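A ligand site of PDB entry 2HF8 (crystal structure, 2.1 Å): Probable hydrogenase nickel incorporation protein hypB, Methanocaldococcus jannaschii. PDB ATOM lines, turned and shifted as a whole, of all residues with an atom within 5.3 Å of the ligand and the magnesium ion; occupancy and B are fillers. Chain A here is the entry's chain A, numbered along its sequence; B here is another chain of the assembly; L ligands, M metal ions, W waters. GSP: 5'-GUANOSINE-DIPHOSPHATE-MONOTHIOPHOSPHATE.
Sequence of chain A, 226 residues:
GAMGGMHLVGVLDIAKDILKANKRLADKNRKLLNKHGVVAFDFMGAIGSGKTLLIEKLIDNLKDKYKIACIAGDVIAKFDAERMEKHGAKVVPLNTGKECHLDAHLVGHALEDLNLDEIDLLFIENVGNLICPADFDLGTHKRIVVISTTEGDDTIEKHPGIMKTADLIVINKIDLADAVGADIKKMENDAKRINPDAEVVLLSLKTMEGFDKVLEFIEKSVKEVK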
ATOM      1  N   ALA A  46      18.556 -28.070 -22.168  1.00  0.00           N
ATOM      2  CA  ALA A  46      17.234 -28.655 -21.977  1.00  0.00           C
ATOM      3  C   ALA A  46      16.622 -28.092 -20.691  1.00  0.00           C
ATOM      4  O   ALA A  46      17.203 -27.215 -20.058  1.00  0.00           O
ATOM      5  CB  ALA A  46      17.336 -30.182 -21.921  1.00  0.00           C
ATOM      6  N   ILE A  47      15.455 -28.601 -20.306  1.00  0.00           N
ATOM      7  CA  ILE A  47      14.792 -28.137 -19.088  1.00  0.00           C
ATOM      8  C   ILE A  47      15.484 -28.695 -17.851  1.00  0.00           C
ATOM      9  O   ILE A  47      15.546 -29.916 -17.685  1.00  0.00           O
ATOM     10  CB  ILE A  47      13.290 -28.529 -19.051  1.00  0.00           C
ATOM     11  CG1 ILE A  47      12.542 -28.048 -20.296  1.00  0.00           C
ATOM     12  CG2 ILE A  47      12.626 -28.042 -17.751  1.00  0.00           C
ATOM     13  CD1 ILE A  47      12.225 -26.574 -20.311  1.00  0.00           C
ATOM     14  N   GLY A  48      15.999 -27.808 -17.008  1.00  0.00           N
ATOM     15  CA  GLY A  48      16.649 -28.192 -15.756  1.00  0.00           C
ATOM     16  C   GLY A  48      18.029 -28.819 -15.871  1.00  0.00           C
ATOM     17  O   GLY A  48      18.503 -29.452 -14.925  1.00  0.00           O
ATOM     18  N   SER A  49      18.666 -28.635 -17.017  1.00  0.00           N
ATOM     19  CA  SER A  49      20.034 -29.114 -17.264  1.00  0.00           C
ATOM     20  C   SER A  49      21.080 -28.536 -16.302  1.00  0.00           C
ATOM     21  O   SER A  49      22.097 -29.183 -16.027  1.00  0.00           O
ATOM     22  CB  SER A  49      20.464 -28.803 -18.692  1.00  0.00           C
ATOM     23  OG  SER A  49      19.721 -29.564 -19.626  1.00  0.00           O
ATOM     24  N   GLY A  50      20.831 -27.325 -15.814  1.00  0.00           N
ATOM     25  CA  GLY A  50      21.710 -26.665 -14.849  1.00  0.00           C
ATOM     26  C   GLY A  50      22.268 -25.311 -15.280  1.00  0.00           C
ATOM     27  O   GLY A  50      23.298 -24.877 -14.748  1.00  0.00           O
ATOM     28  N   LYS A  51      21.586 -24.651 -16.207  1.00  0.00           N
ATOM     29  CA  LYS A  51      22.007 -23.335 -16.732  1.00  0.00           C
ATOM     30  C   LYS A  51      22.150 -22.268 -15.638  1.00  0.00           C
ATOM     31  O   LYS A  51      23.184 -21.605 -15.554  1.00  0.00           O
ATOM     32  CB  LYS A  51      21.028 -22.825 -17.813  1.00  0.00           C
ATOM     33  CG  LYS A  51      20.869 -23.727 -19.043  1.00  0.00           C
ATOM     34  CD  LYS A  51      19.855 -23.160 -20.059  1.00  0.00           C
ATOM     35  CE  LYS A  51      18.392 -23.341 -19.640  1.00  0.00           C
ATOM     36  NZ  LYS A  51      18.069 -24.716 -19.156  1.00  0.00           N
ATOM     37  N   THR A  52      21.120 -22.123 -14.812  1.00  0.00           N
ATOM     38  CA  THR A  52      21.132 -21.125 -13.730  1.00  0.00           C
ATOM     39  C   THR A  52      22.234 -21.406 -12.705  1.00  0.00           C
ATOM     40  O   THR A  52      22.991 -20.495 -12.351  1.00  0.00           O
ATOM     41  CB  THR A  52      19.757 -21.008 -13.034  1.00  0.00           C
ATOM     42  OG1 THR A  52      18.735 -20.794 -14.031  1.00  0.00           O
ATOM     43  CG2 THR A  52      19.734 -19.844 -12.051  1.00  0.00           C
ATOM     44  N   LEU A  53      22.358 -22.657 -12.272  1.00  0.00           N
ATOM     45  CA  LEU A  53      23.367 -23.025 -11.275  1.00  0.00           C
ATOM     46  C   LEU A  53      24.787 -22.812 -11.815  1.00  0.00           C
ATOM     47  O   LEU A  53      25.672 -22.405 -11.079  1.00  0.00           O
ATOM     48  CB  LEU A  53      23.181 -24.470 -10.762  1.00  0.00           C
ATOM     49  CG  LEU A  53      24.022 -24.914  -9.555  1.00  0.00           C
ATOM     50  CD1 LEU A  53      23.808 -23.995  -8.350  1.00  0.00           C
ATOM     51  CD2 LEU A  53      23.741 -26.376  -9.163  1.00  0.00           C
ATOM     52  N   LEU A  54      24.978 -23.070 -13.113  1.00  0.00           N
ATOM     53  CA  LEU A  54      26.261 -22.841 -13.762  1.00  0.00           C
ATOM     54  C   LEU A  54      26.591 -21.343 -13.759  1.00  0.00           C
ATOM     55  O   LEU A  54      27.695 -20.960 -13.396  1.00  0.00           O
ATOM     56  CB  LEU A  54      26.272 -23.393 -15.200  1.00  0.00           C
ATOM     57  CG  LEU A  54      27.532 -23.144 -16.046  1.00  0.00           C
ATOM     58  CD1 LEU A  54      28.800 -23.703 -15.411  1.00  0.00           C
ATOM     59  CD2 LEU A  54      27.362 -23.662 -17.490  1.00  0.00           C
ATOM     60  N   ASP A  74      12.756 -16.718 -19.748  1.00  0.00           N
ATOM     61  CA  ASP A  74      11.898 -17.881 -19.524  1.00  0.00           C
ATOM     62  C   ASP A  74      10.431 -17.465 -19.474  1.00  0.00           C
ATOM     63  O   ASP A  74      10.116 -16.283 -19.369  1.00  0.00           O
ATOM     64  CB  ASP A  74      12.279 -18.610 -18.236  1.00  0.00           C
ATOM     65  CG  ASP A  74      11.954 -20.088 -18.259  1.00  0.00           C
ATOM     66  OD1 ASP A  74      11.322 -20.585 -19.230  1.00  0.00           O
ATOM     67  OD2 ASP A  74      12.315 -20.774 -17.292  1.00  0.00           O
ATOM     68  N   ASP A  80      14.612 -17.390 -11.980  1.00  0.00           N
ATOM     69  CA  ASP A  80      16.041 -17.402 -12.234  1.00  0.00           C
ATOM     70  C   ASP A  80      16.661 -16.025 -12.089  1.00  0.00           C
ATOM     71  O   ASP A  80      17.812 -15.918 -11.697  1.00  0.00           O
ATOM     72  CB  ASP A  80      16.327 -18.001 -13.602  1.00  0.00           C
ATOM     73  CG  ASP A  80      16.048 -19.491 -13.644  1.00  0.00           C
ATOM     74  OD1 ASP A  80      15.702 -20.075 -12.592  1.00  0.00           O
ATOM     75  OD2 ASP A  80      16.210 -20.101 -14.717  1.00  0.00           O
ATOM     76  N   ARG A  83      17.427 -15.699  -8.448  1.00  0.00           N
ATOM     77  CA  ARG A  83      18.606 -16.519  -8.136  1.00  0.00           C
ATOM     78  C   ARG A  83      19.920 -15.831  -8.489  1.00  0.00           C
ATOM     79  O   ARG A  83      20.842 -15.794  -7.669  1.00  0.00           O
ATOM     80  CB  ARG A  83      18.507 -17.903  -8.793  1.00  0.00           C
ATOM     81  CG  ARG A  83      17.720 -18.901  -7.946  1.00  0.00           C
ATOM     82  CD  ARG A  83      17.463 -20.215  -8.670  1.00  0.00           C
ATOM     83  NE  ARG A  83      18.679 -20.992  -8.892  1.00  0.00           N
ATOM     84  CZ  ARG A  83      18.736 -22.140  -9.563  1.00  0.00           C
ATOM     85  NH1 ARG A  83      17.643 -22.670 -10.083  1.00  0.00           N
ATOM     86  NH2 ARG A  83      19.904 -22.754  -9.722  1.00  0.00           N
ATOM     87  N   GLU A 125      20.856 -16.416 -20.084  1.00  0.00           N
ATOM     88  CA  GLU A 125      20.193 -17.709 -19.982  1.00  0.00           C
ATOM     89  C   GLU A 125      19.004 -17.768 -20.925  1.00  0.00           C
ATOM     90  O   GLU A 125      18.023 -17.043 -20.758  1.00  0.00           O
ATOM     91  CB  GLU A 125      19.782 -18.074 -18.560  1.00  0.00           C
ATOM     92  CG  GLU A 125      19.338 -19.540 -18.463  1.00  0.00           C
ATOM     93  CD  GLU A 125      18.988 -19.963 -17.060  1.00  0.00           C
ATOM     94  OE1 GLU A 125      19.532 -19.360 -16.121  1.00  0.00           O
ATOM     95  OE2 GLU A 125      18.165 -20.888 -16.889  1.00  0.00           O
ATOM     96  N   GLY A 128      14.738 -22.959 -21.734  1.00  0.00           N
ATOM     97  CA  GLY A 128      15.004 -24.397 -21.737  1.00  0.00           C
ATOM     98  C   GLY A 128      14.331 -25.058 -22.926  1.00  0.00           C
ATOM     99  O   GLY A 128      13.102 -25.180 -22.955  1.00  0.00           O
ATOM    100  N   ASN A 172      26.420 -32.100 -17.928  1.00  0.00           N
ATOM    101  CA  ASN A 172      26.339 -31.777 -16.499  1.00  0.00           C
ATOM    102  C   ASN A 172      25.714 -32.930 -15.715  1.00  0.00           C
ATOM    103  O   ASN A 172      25.244 -33.906 -16.304  1.00  0.00           O
ATOM    104  CB  ASN A 172      25.536 -30.470 -16.326  1.00  0.00           C
ATOM    105  CG  ASN A 172      25.584 -29.926 -14.900  1.00  0.00           C
ATOM    106  OD1 ASN A 172      24.585 -29.397 -14.398  1.00  0.00           O
ATOM    107  ND2 ASN A 172      26.727 -30.045 -14.238  1.00  0.00           N
ATOM    108  N   LYS A 173      25.732 -32.822 -14.385  1.00  0.00           N
ATOM    109  CA  LYS A 173      25.209 -33.853 -13.458  1.00  0.00           C
ATOM    110  C   LYS A 173      25.881 -35.207 -13.671  1.00  0.00           C
ATOM    111  O   LYS A 173      25.205 -36.242 -13.635  1.00  0.00           O
ATOM    112  CB  LYS A 173      23.686 -34.001 -13.572  1.00  0.00           C
ATOM    113  CG  LYS A 173      22.895 -32.721 -13.391  1.00  0.00           C
ATOM    114  CD  LYS A 173      21.397 -32.983 -13.428  1.00  0.00           C
ATOM    115  CE  LYS A 173      20.626 -31.715 -13.722  1.00  0.00           C
ATOM    116  NZ  LYS A 173      19.354 -32.022 -14.456  1.00  0.00           N
ATOM    117  N   ILE A 174      27.190 -35.210 -13.877  1.00  0.00           N
ATOM    118  CA  ILE A 174      27.905 -36.475 -14.034  1.00  0.00           C
ATOM    119  C   ILE A 174      27.849 -37.327 -12.761  1.00  0.00           C
ATOM    120  O   ILE A 174      27.991 -38.536 -12.839  1.00  0.00           O
ATOM    121  CB  ILE A 174      29.372 -36.308 -14.544  1.00  0.00           C
ATOM    122  CG1 ILE A 174      30.223 -35.490 -13.566  1.00  0.00           C
ATOM    123  CG2 ILE A 174      29.394 -35.774 -15.999  1.00  0.00           C
ATOM    124  CD1 ILE A 174      31.713 -35.448 -13.930  1.00  0.00           C
ATOM    125  N   ASP A 175      27.621 -36.671 -11.621  1.00  0.00           N
ATOM    126  CA  ASP A 175      27.435 -37.374 -10.341  1.00  0.00           C
ATOM    127  C   ASP A 175      26.200 -38.283 -10.306  1.00  0.00           C
ATOM    128  O   ASP A 175      26.120 -39.179  -9.470  1.00  0.00           O
ATOM    129  CB  ASP A 175      27.418 -36.391  -9.152  1.00  0.00           C
ATOM    130  CG  ASP A 175      26.325 -35.340  -9.271  1.00  0.00           C
ATOM    131  OD1 ASP A 175      26.411 -34.466 -10.167  1.00  0.00           O
ATOM    132  OD2 ASP A 175      25.393 -35.349  -8.437  1.00  0.00           O
ATOM    133  N   LEU A 176      25.264 -38.053 -11.225  1.00  0.00           N
ATOM    134  CA  LEU A 176      24.005 -38.815 -11.254  1.00  0.00           C
ATOM    135  C   LEU A 176      23.927 -39.857 -12.377  1.00  0.00           C
ATOM    136  O   LEU A 176      22.884 -40.491 -12.565  1.00  0.00           O
ATOM    137  CB  LEU A 176      22.811 -37.849 -11.373  1.00  0.00           C
ATOM    138  CG  LEU A 176      22.694 -36.744 -10.323  1.00  0.00           C
ATOM    139  CD1 LEU A 176      21.482 -35.887 -10.579  1.00  0.00           C
ATOM    140  CD2 LEU A 176      22.659 -37.324  -8.914  1.00  0.00           C
ATOM    141  N   LEU A 203      30.896 -32.242 -16.450  1.00  0.00           N
ATOM    142  CA  LEU A 203      30.736 -31.392 -15.276  1.00  0.00           C
ATOM    143  C   LEU A 203      29.822 -32.006 -14.217  1.00  0.00           C
ATOM    144  O   LEU A 203      28.841 -32.669 -14.535  1.00  0.00           O
ATOM    145  CB  LEU A 203      30.148 -30.032 -15.711  1.00  0.00           C
ATOM    146  CG  LEU A 203      29.908 -28.904 -14.692  1.00  0.00           C
ATOM    147  CD1 LEU A 203      31.215 -28.393 -14.082  1.00  0.00           C
ATOM    148  CD2 LEU A 203      29.148 -27.740 -15.331  1.00  0.00           C
ATOM    149  N   SER A 204      30.167 -31.765 -12.949  1.00  0.00           N
ATOM    150  CA  SER A 204      29.196 -31.821 -11.882  1.00  0.00           C
ATOM    151  C   SER A 204      29.237 -30.513 -11.123  1.00  0.00           C
ATOM    152  O   SER A 204      30.279 -30.113 -10.610  1.00  0.00           O
ATOM    153  CB  SER A 204      29.453 -32.989 -10.925  1.00  0.00           C
ATOM    154  OG  SER A 204      28.572 -32.904  -9.808  1.00  0.00           O
ATOM    155  N   LEU A 205      28.088 -29.840 -11.061  1.00  0.00           N
ATOM    156  CA  LEU A 205      27.955 -28.619 -10.272  1.00  0.00           C
ATOM    157  C   LEU A 205      27.738 -28.910  -8.787  1.00  0.00           C
ATOM    158  O   LEU A 205      27.797 -28.003  -7.958  1.00  0.00           O
ATOM    159  CB  LEU A 205      26.839 -27.726 -10.847  1.00  0.00           C
ATOM    160  CG  LEU A 205      27.186 -27.067 -12.185  1.00  0.00           C
ATOM    161  CD1 LEU A 205      25.957 -26.436 -12.841  1.00  0.00           C
ATOM    162  CD2 LEU A 205      28.319 -26.039 -12.035  1.00  0.00           C
ATOM    163  N   LYS A 206      27.491 -30.168  -8.460  1.00  0.00           N
ATOM    164  CA  LYS A 206      27.429 -30.628  -7.065  1.00  0.00           C
ATOM    165  C   LYS A 206      28.840 -30.827  -6.486  1.00  0.00           C
ATOM    166  O   LYS A 206      29.161 -30.264  -5.435  1.00  0.00           O
ATOM    167  CB  LYS A 206      26.599 -31.899  -6.956  1.00  0.00           C
ATOM    168  CG  LYS A 206      26.308 -32.368  -5.532  1.00  0.00           C
ATOM    169  CD  LYS A 206      25.298 -33.499  -5.547  1.00  0.00           C
ATOM    170  CE  LYS A 206      24.716 -33.790  -4.171  1.00  0.00           C
ATOM    171  NZ  LYS A 206      23.685 -34.870  -4.253  1.00  0.00           N
ATOM    172  N   THR B 149      11.943 -34.810 -11.168  1.00  0.00           N
ATOM    173  CA  THR B 149      12.569 -34.071 -10.068  1.00  0.00           C
ATOM    174  C   THR B 149      13.914 -33.474 -10.461  1.00  0.00           C
ATOM    175  O   THR B 149      14.289 -32.414  -9.957  1.00  0.00           O
ATOM    176  CB  THR B 149      12.777 -34.970  -8.829  1.00  0.00           C
ATOM    177  OG1 THR B 149      13.667 -36.047  -9.147  1.00  0.00           O
ATOM    178  CG2 THR B 149      11.449 -35.522  -8.309  1.00  0.00           C
ATOM    179  N   THR B 150      14.622 -34.149 -11.360  1.00  0.00           N
ATOM    180  CA  THR B 150      15.975 -33.750 -11.769  1.00  0.00           C
ATOM    181  C   THR B 150      16.004 -32.481 -12.632  1.00  0.00           C
ATOM    182  O   THR B 150      17.067 -31.913 -12.889  1.00  0.00           O
ATOM    183  CB  THR B 150      16.724 -34.912 -12.485  1.00  0.00           C
ATOM    184  OG1 THR B 150      15.991 -35.328 -13.635  1.00  0.00           O
ATOM    185  CG2 THR B 150      16.908 -36.093 -11.540  1.00  0.00           C
ATOM    186  N   GLU B 151      14.825 -32.046 -13.062  1.00  0.00           N
ATOM    187  CA  GLU B 151      14.688 -30.771 -13.746  1.00  0.00           C
ATOM    188  C   GLU B 151      14.607 -29.598 -12.751  1.00  0.00           C
ATOM    189  O   GLU B 151      14.662 -28.434 -13.150  1.00  0.00           O
ATOM    190  CB  GLU B 151      13.450 -30.794 -14.648  1.00  0.00           C
ATOM    191  CG  GLU B 151      13.551 -31.812 -15.790  1.00  0.00           C
ATOM    192  CD  GLU B 151      12.225 -32.507 -16.082  1.00  0.00           C
ATOM    193  OE1 GLU B 151      11.153 -31.927 -15.809  1.00  0.00           O
ATOM    194  OE2 GLU B 151      12.268 -33.655 -16.577  1.00  0.00           O
ATOM    195  N   GLY B 152      14.502 -29.898 -11.453  1.00  0.00           N
ATOM    196  CA  GLY B 152      14.368 -28.857 -10.429  1.00  0.00           C
ATOM    197  C   GLY B 152      12.932 -28.720  -9.969  1.00  0.00           C
ATOM    198  O   GLY B 152      12.009 -28.971 -10.735  1.00  0.00           O
ATOM    199  N   ASP B 153      12.729 -28.306  -8.715  1.00  0.00           N
ATOM    200  CA  ASP B 153      11.382 -28.268  -8.136  1.00  0.00           C
ATOM    201  C   ASP B 153      10.583 -27.004  -8.451  1.00  0.00           C
ATOM    202  O   ASP B 153       9.457 -26.846  -7.977  1.00  0.00           O
ATOM    203  CB  ASP B 153      11.384 -28.600  -6.621  1.00  0.00           C
ATOM    204  CG  ASP B 153      12.233 -27.651  -5.798  1.00  0.00           C
ATOM    205  OD1 ASP B 153      12.483 -26.501  -6.227  1.00  0.00           O
ATOM    206  OD2 ASP B 153      12.657 -28.061  -4.681  1.00  0.00           O
ATOM    207  N   THR B 155      10.057 -26.401 -11.729  1.00  0.00           N
ATOM    208  CA  THR B 155       9.647 -26.736 -13.103  1.00  0.00           C
ATOM    209  C   THR B 155       8.136 -26.639 -13.338  1.00  0.00           C
ATOM    210  O   THR B 155       7.695 -26.177 -14.390  1.00  0.00           O
ATOM    211  CB  THR B 155      10.162 -28.150 -13.514  1.00  0.00           C
ATOM    212  OG1 THR B 155      11.591 -28.178 -13.425  1.00  0.00           O
ATOM    213  CG2 THR B 155       9.760 -28.494 -14.945  1.00  0.00           C
ATOM    214  N   LYS B 158       6.993 -22.929 -13.079  1.00  0.00           N
ATOM    215  CA  LYS B 158       7.598 -22.235 -14.225  1.00  0.00           C
ATOM    216  C   LYS B 158       6.837 -22.447 -15.537  1.00  0.00           C
ATOM    217  O   LYS B 158       7.049 -21.705 -16.504  1.00  0.00           O
ATOM    218  CB  LYS B 158       9.046 -22.687 -14.434  1.00  0.00           C
ATOM    219  CG  LYS B 158      10.072 -22.024 -13.526  1.00  0.00           C
ATOM    220  CD  LYS B 158      11.468 -22.517 -13.878  1.00  0.00           C
ATOM    221  CE  LYS B 158      12.507 -21.979 -12.927  1.00  0.00           C
ATOM    222  NZ  LYS B 158      13.873 -22.416 -13.362  1.00  0.00           N
ATOM    223  N   HIS B 159       5.971 -23.457 -15.577  1.00  0.00           N
ATOM    224  CA  HIS B 159       5.250 -23.786 -16.811  1.00  0.00           C
ATOM    225  C   HIS B 159       3.754 -24.028 -16.589  1.00  0.00           C
ATOM    226  O   HIS B 159       3.250 -25.110 -16.919  1.00  0.00           O
ATOM    227  CB  HIS B 159       5.891 -25.002 -17.498  1.00  0.00           C
ATOM    228  CG  HIS B 159       7.369 -24.877 -17.716  1.00  0.00           C
ATOM    229  ND1 HIS B 159       8.289 -25.367 -16.811  1.00  0.00           N
ATOM    230  CD2 HIS B 159       8.080 -24.308 -18.714  1.00  0.00           C
ATOM    231  CE1 HIS B 159       9.503 -25.112 -17.256  1.00  0.00           C
ATOM    232  NE2 HIS B 159       9.407 -24.471 -18.412  1.00  0.00           N
ATOM    233  N   ALA B 179      19.080 -36.136  -4.381  1.00  0.00           N
ATOM    234  CA  ALA B 179      20.340 -35.899  -5.099  1.00  0.00           C
ATOM    235  C   ALA B 179      20.418 -34.533  -5.798  1.00  0.00           C
ATOM    236  O   ALA B 179      21.503 -33.945  -5.890  1.00  0.00           O
ATOM    237  CB  ALA B 179      20.580 -37.023  -6.105  1.00  0.00           C
ATOM    238  N   VAL B 180      19.280 -34.037  -6.288  1.00  0.00           N
ATOM    239  CA  VAL B 180      19.216 -32.715  -6.947  1.00  0.00           C
ATOM    240  C   VAL B 180      18.696 -31.605  -6.030  1.00  0.00           C
ATOM    241  O   VAL B 180      18.608 -30.445  -6.422  1.00  0.00           O
ATOM    242  CB  VAL B 180      18.366 -32.749  -8.253  1.00  0.00           C
ATOM    243  CG1 VAL B 180      19.087 -33.496  -9.366  1.00  0.00           C
ATOM    244  CG2 VAL B 180      16.985 -33.341  -7.994  1.00  0.00           C
ATOM    245  N   GLY B 181      18.339 -31.974  -4.797  1.00  0.00           N
ATOM    246  CA  GLY B 181      17.786 -31.015  -3.844  1.00  0.00           C
ATOM    247  C   GLY B 181      16.329 -30.633  -4.101  1.00  0.00           C
ATOM    248  O   GLY B 181      15.873 -29.578  -3.638  1.00  0.00           O
ATOM    249  N   ALA B 182      15.598 -31.485  -4.810  1.00  0.00           N
ATOM    250  CA  ALA B 182      14.181 -31.225  -5.135  1.00  0.00           C
ATOM    251  C   ALA B 182      13.229 -31.593  -4.000  1.00  0.00           C
ATOM    252  O   ALA B 182      13.331 -32.667  -3.404  1.00  0.00           O
ATOM    253  CB  ALA B 182      13.789 -31.954  -6.411  1.00  0.00           C
HETATM  254  PG  GSP L   1      15.523 -24.112 -16.154  1.00  0.00           P
HETATM  255  O3B GSP L   1      16.594 -25.048 -15.414  1.00  0.00           O
HETATM  256  S1G GSP L   1      15.288 -24.632 -17.767  1.00  0.00           S
HETATM  257  O2G GSP L   1      14.178 -24.256 -15.391  1.00  0.00           O
HETATM  258  O3G GSP L   1      15.994 -22.653 -16.160  1.00  0.00           O
HETATM  259  PB  GSP L   1      18.189 -24.833 -15.377  1.00  0.00           P
HETATM  260  O1B GSP L   1      18.806 -25.384 -16.600  1.00  0.00           O
HETATM  261  O2B GSP L   1      18.576 -23.417 -15.158  1.00  0.00           O
HETATM  262  PA  GSP L   1      18.886 -25.351 -12.658  1.00  0.00           P
HETATM  263  O1A GSP L   1      20.136 -24.561 -12.504  1.00  0.00           O
HETATM  264  O2A GSP L   1      17.700 -24.636 -12.138  1.00  0.00           O
HETATM  265  O3A GSP L   1      18.643 -25.790 -14.176  1.00  0.00           O
HETATM  266  O5' GSP L   1      19.097 -26.787 -11.979  1.00  0.00           O
HETATM  267  C5' GSP L   1      18.083 -27.764 -12.009  1.00  0.00           C
HETATM  268  C4' GSP L   1      18.260 -28.719 -10.821  1.00  0.00           C
HETATM  269  O4' GSP L   1      19.403 -29.523 -10.999  1.00  0.00           O
HETATM  270  C3' GSP L   1      18.469 -28.000  -9.493  1.00  0.00           C
HETATM  271  O3' GSP L   1      17.776 -28.788  -8.550  1.00  0.00           O
HETATM  272  C2' GSP L   1      19.965 -28.080  -9.256  1.00  0.00           C
HETATM  273  O2' GSP L   1      20.301 -28.108  -7.889  1.00  0.00           O
HETATM  274  C1' GSP L   1      20.296 -29.407  -9.893  1.00  0.00           C
HETATM  275  N9  GSP L   1      21.646 -29.565 -10.445  1.00  0.00           N
HETATM  276  C8  GSP L   1      22.254 -28.793 -11.407  1.00  0.00           C
HETATM  277  N7  GSP L   1      23.473 -29.334 -11.652  1.00  0.00           N
HETATM  278  C5  GSP L   1      23.627 -30.439 -10.892  1.00  0.00           C
HETATM  279  C6  GSP L   1      24.656 -31.369 -10.765  1.00  0.00           C
HETATM  280  O6  GSP L   1      25.683 -31.237 -11.426  1.00  0.00           O
HETATM  281  N1  GSP L   1      24.527 -32.426  -9.876  1.00  0.00           N
HETATM  282  C2  GSP L   1      23.374 -32.563  -9.133  1.00  0.00           C
HETATM  283  N2  GSP L   1      23.244 -33.585  -8.291  1.00  0.00           N
HETATM  284  N3  GSP L   1      22.360 -31.650  -9.263  1.00  0.00           N
HETATM  285  C4  GSP L   1      22.478 -30.605 -10.127  1.00  0.00           C
HETATM  286 MG    MG M   1      17.339 -21.696 -15.155  1.00  0.00          MG
HETATM  287  O   HOH W   1      15.330 -28.201  -7.248  1.00  0.00           O
HETATM  288  O   HOH W   2      16.637 -22.433 -13.381  1.00  0.00           O
HETATM  289  O   HOH W   3      12.226 -23.428 -17.446  1.00  0.00           O
HETATM  290  O   HOH W   4      22.396 -29.787  -6.515  1.00  0.00           O
HETATM  291  O   HOH W   5      12.004 -25.905 -15.328  1.00  0.00           O
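N7 of the ligand sits close to OD1 of Asn 172 (3.0 Å). An oxygen (O1A) of the ligand lies within hydrogen-bond range of the backbone NH (N) of Thr 52, at 3.5 Å. O1B of the ligand lies within hydrogen-bond range of N of Ser 49 (3.3 Å). A nitrogen (N2) of the ligand is in hydrogen-bond range of the side-chain carboxylate (OD2) of Asp 175 (2.8 Å). N of Lys 173 lies close to O6 of the ligand (3.4 Å). The backbone NH of Leu 205 lies within hydrogen-bond range of an oxygen (O6) of the ligand, at 2.8 Å. NZ of Lys 51 lies within salt-bridge range of O1B of the ligand (2.7 Å). The backbone carbonyl oxygen of Ala 179 of chain B sits at hydrogen-bond distance from a nitrogen (N2) of the ligand (3.0 Å). N of Gly 48 lies close to O3B of the ligand (3.2 Å). An oxygen (O2G) of the ligand is in hydrogen-bond range of the side-chain amino group (NZ) of Lys 158 of chain B, 2.8 Å away. N of Gly 50 sits at hydrogen-bond distance from O1B of the ligand. The backbone NH of Lys 51 lies within hydrogen-bond range of an oxygen (O1B) of the ligand (2.9 Å). The backbone NH (N) of Leu 53 lies within hydrogen-bond range of an oxygen (O1A) of the ligand (2.9 Å). NH1 of Arg 83 is in salt-bridge range of O2A of the ligand (2.8 Å). O of Val 180 of chain B sits at hydrogen-bond distance from O3' of the ligand (2.8 Å).
OG1 of Thr 155 of chain B lies within hydrogen-bond range of O of Gly 152 of chain B, at 2.8 Å. The side-chain carboxylate (OD1) of Asp 175 sits at hydrogen-bond distance from the side-chain hydroxyl (OG) of Ser 204 (2.7 Å). The backbone carbonyl oxygen (O) of Ala 179 of chain B lies within hydrogen-bond range of the side-chain amino group (NZ) of Lys 206 (2.9 Å). OG of Ser 49 sits at hydrogen-bond distance from N of Ala 46, 3.2 Å away. The backbone NH of Leu 205 sits close to the side-chain amide nitrogen of Asn 172 (3.5 Å). The side-chain hydroxyl of Ser 204 lies close to the backbone NH of Lys 206 (3.2 Å). The side-chain amino group of Lys 173 is in hydrogen-bond range of the backbone carbonyl oxygen of Thr 150 of chain B, 2.8 Å away. The backbone carbonyl oxygen of Ser 49 sits close to the side-chain amide oxygen of Asn 172 (3.0 Å).
Merely in contact with the ligand: Ala 46, Ile 47, Gly 128, Leu 176, Ser 204, Lys 206, Thr 150 of chain B, Glu 151 of chain B and Gly 152 of chain B. Hydrophobic or aromatic side chains within 4 Å of the ligand: Leu 53, Leu 176, Leu 205 and Val 180 of chain B. Of the 35 residues printed, 25 come within 4 Å of the ligand.
Merely in contact with the magnesium ion: Lys 158 of chain B (3.97 Å). Four residues have an atom within 4 Å of the magnesium ion: Thr 52, Asp 80, Glu 125 and Lys 158 of chain B. The nearest printed residue that does not touch the magnesium ion is Lys 51 (4.7 Å).
The magnesium ion is bound by an oxygen (O3G) of the ligand (1.9 Å), the side-chain carboxylate (OD2) of Asp 80 (2.0 Å), the side-chain hydroxyl (OG1) of Thr 52 (2.0 Å), water W2 (2.0 Å), the side-chain carboxylate (OE2) of Glu 125 (2.1 Å) and an oxygen (O2B) of the ligand (2.1 Å).
Water W2 lies within hydrogen-bond range of the side-chain carboxylate of Asp 80 (2.7 Å), an oxygen (O2A) of the ligand (2.7 Å), the side-chain amino group of Lys 158 of chain B (2.8 Å) and the guanidinium group of Arg 83 (3.5 Å). Water W5 lies within hydrogen-bond range of O2G of the ligand and OG1 of Thr 155 of chain B. Water W1 bridges an oxygen (O3') of the ligand (2.8 Å) and the backbone NH of Asp 153 of chain B (3.0 Å). Water W3 lies within hydrogen-bond range of OD2 of Asp 74, O2G of the ligand and NE2 of His 159 of chain B.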
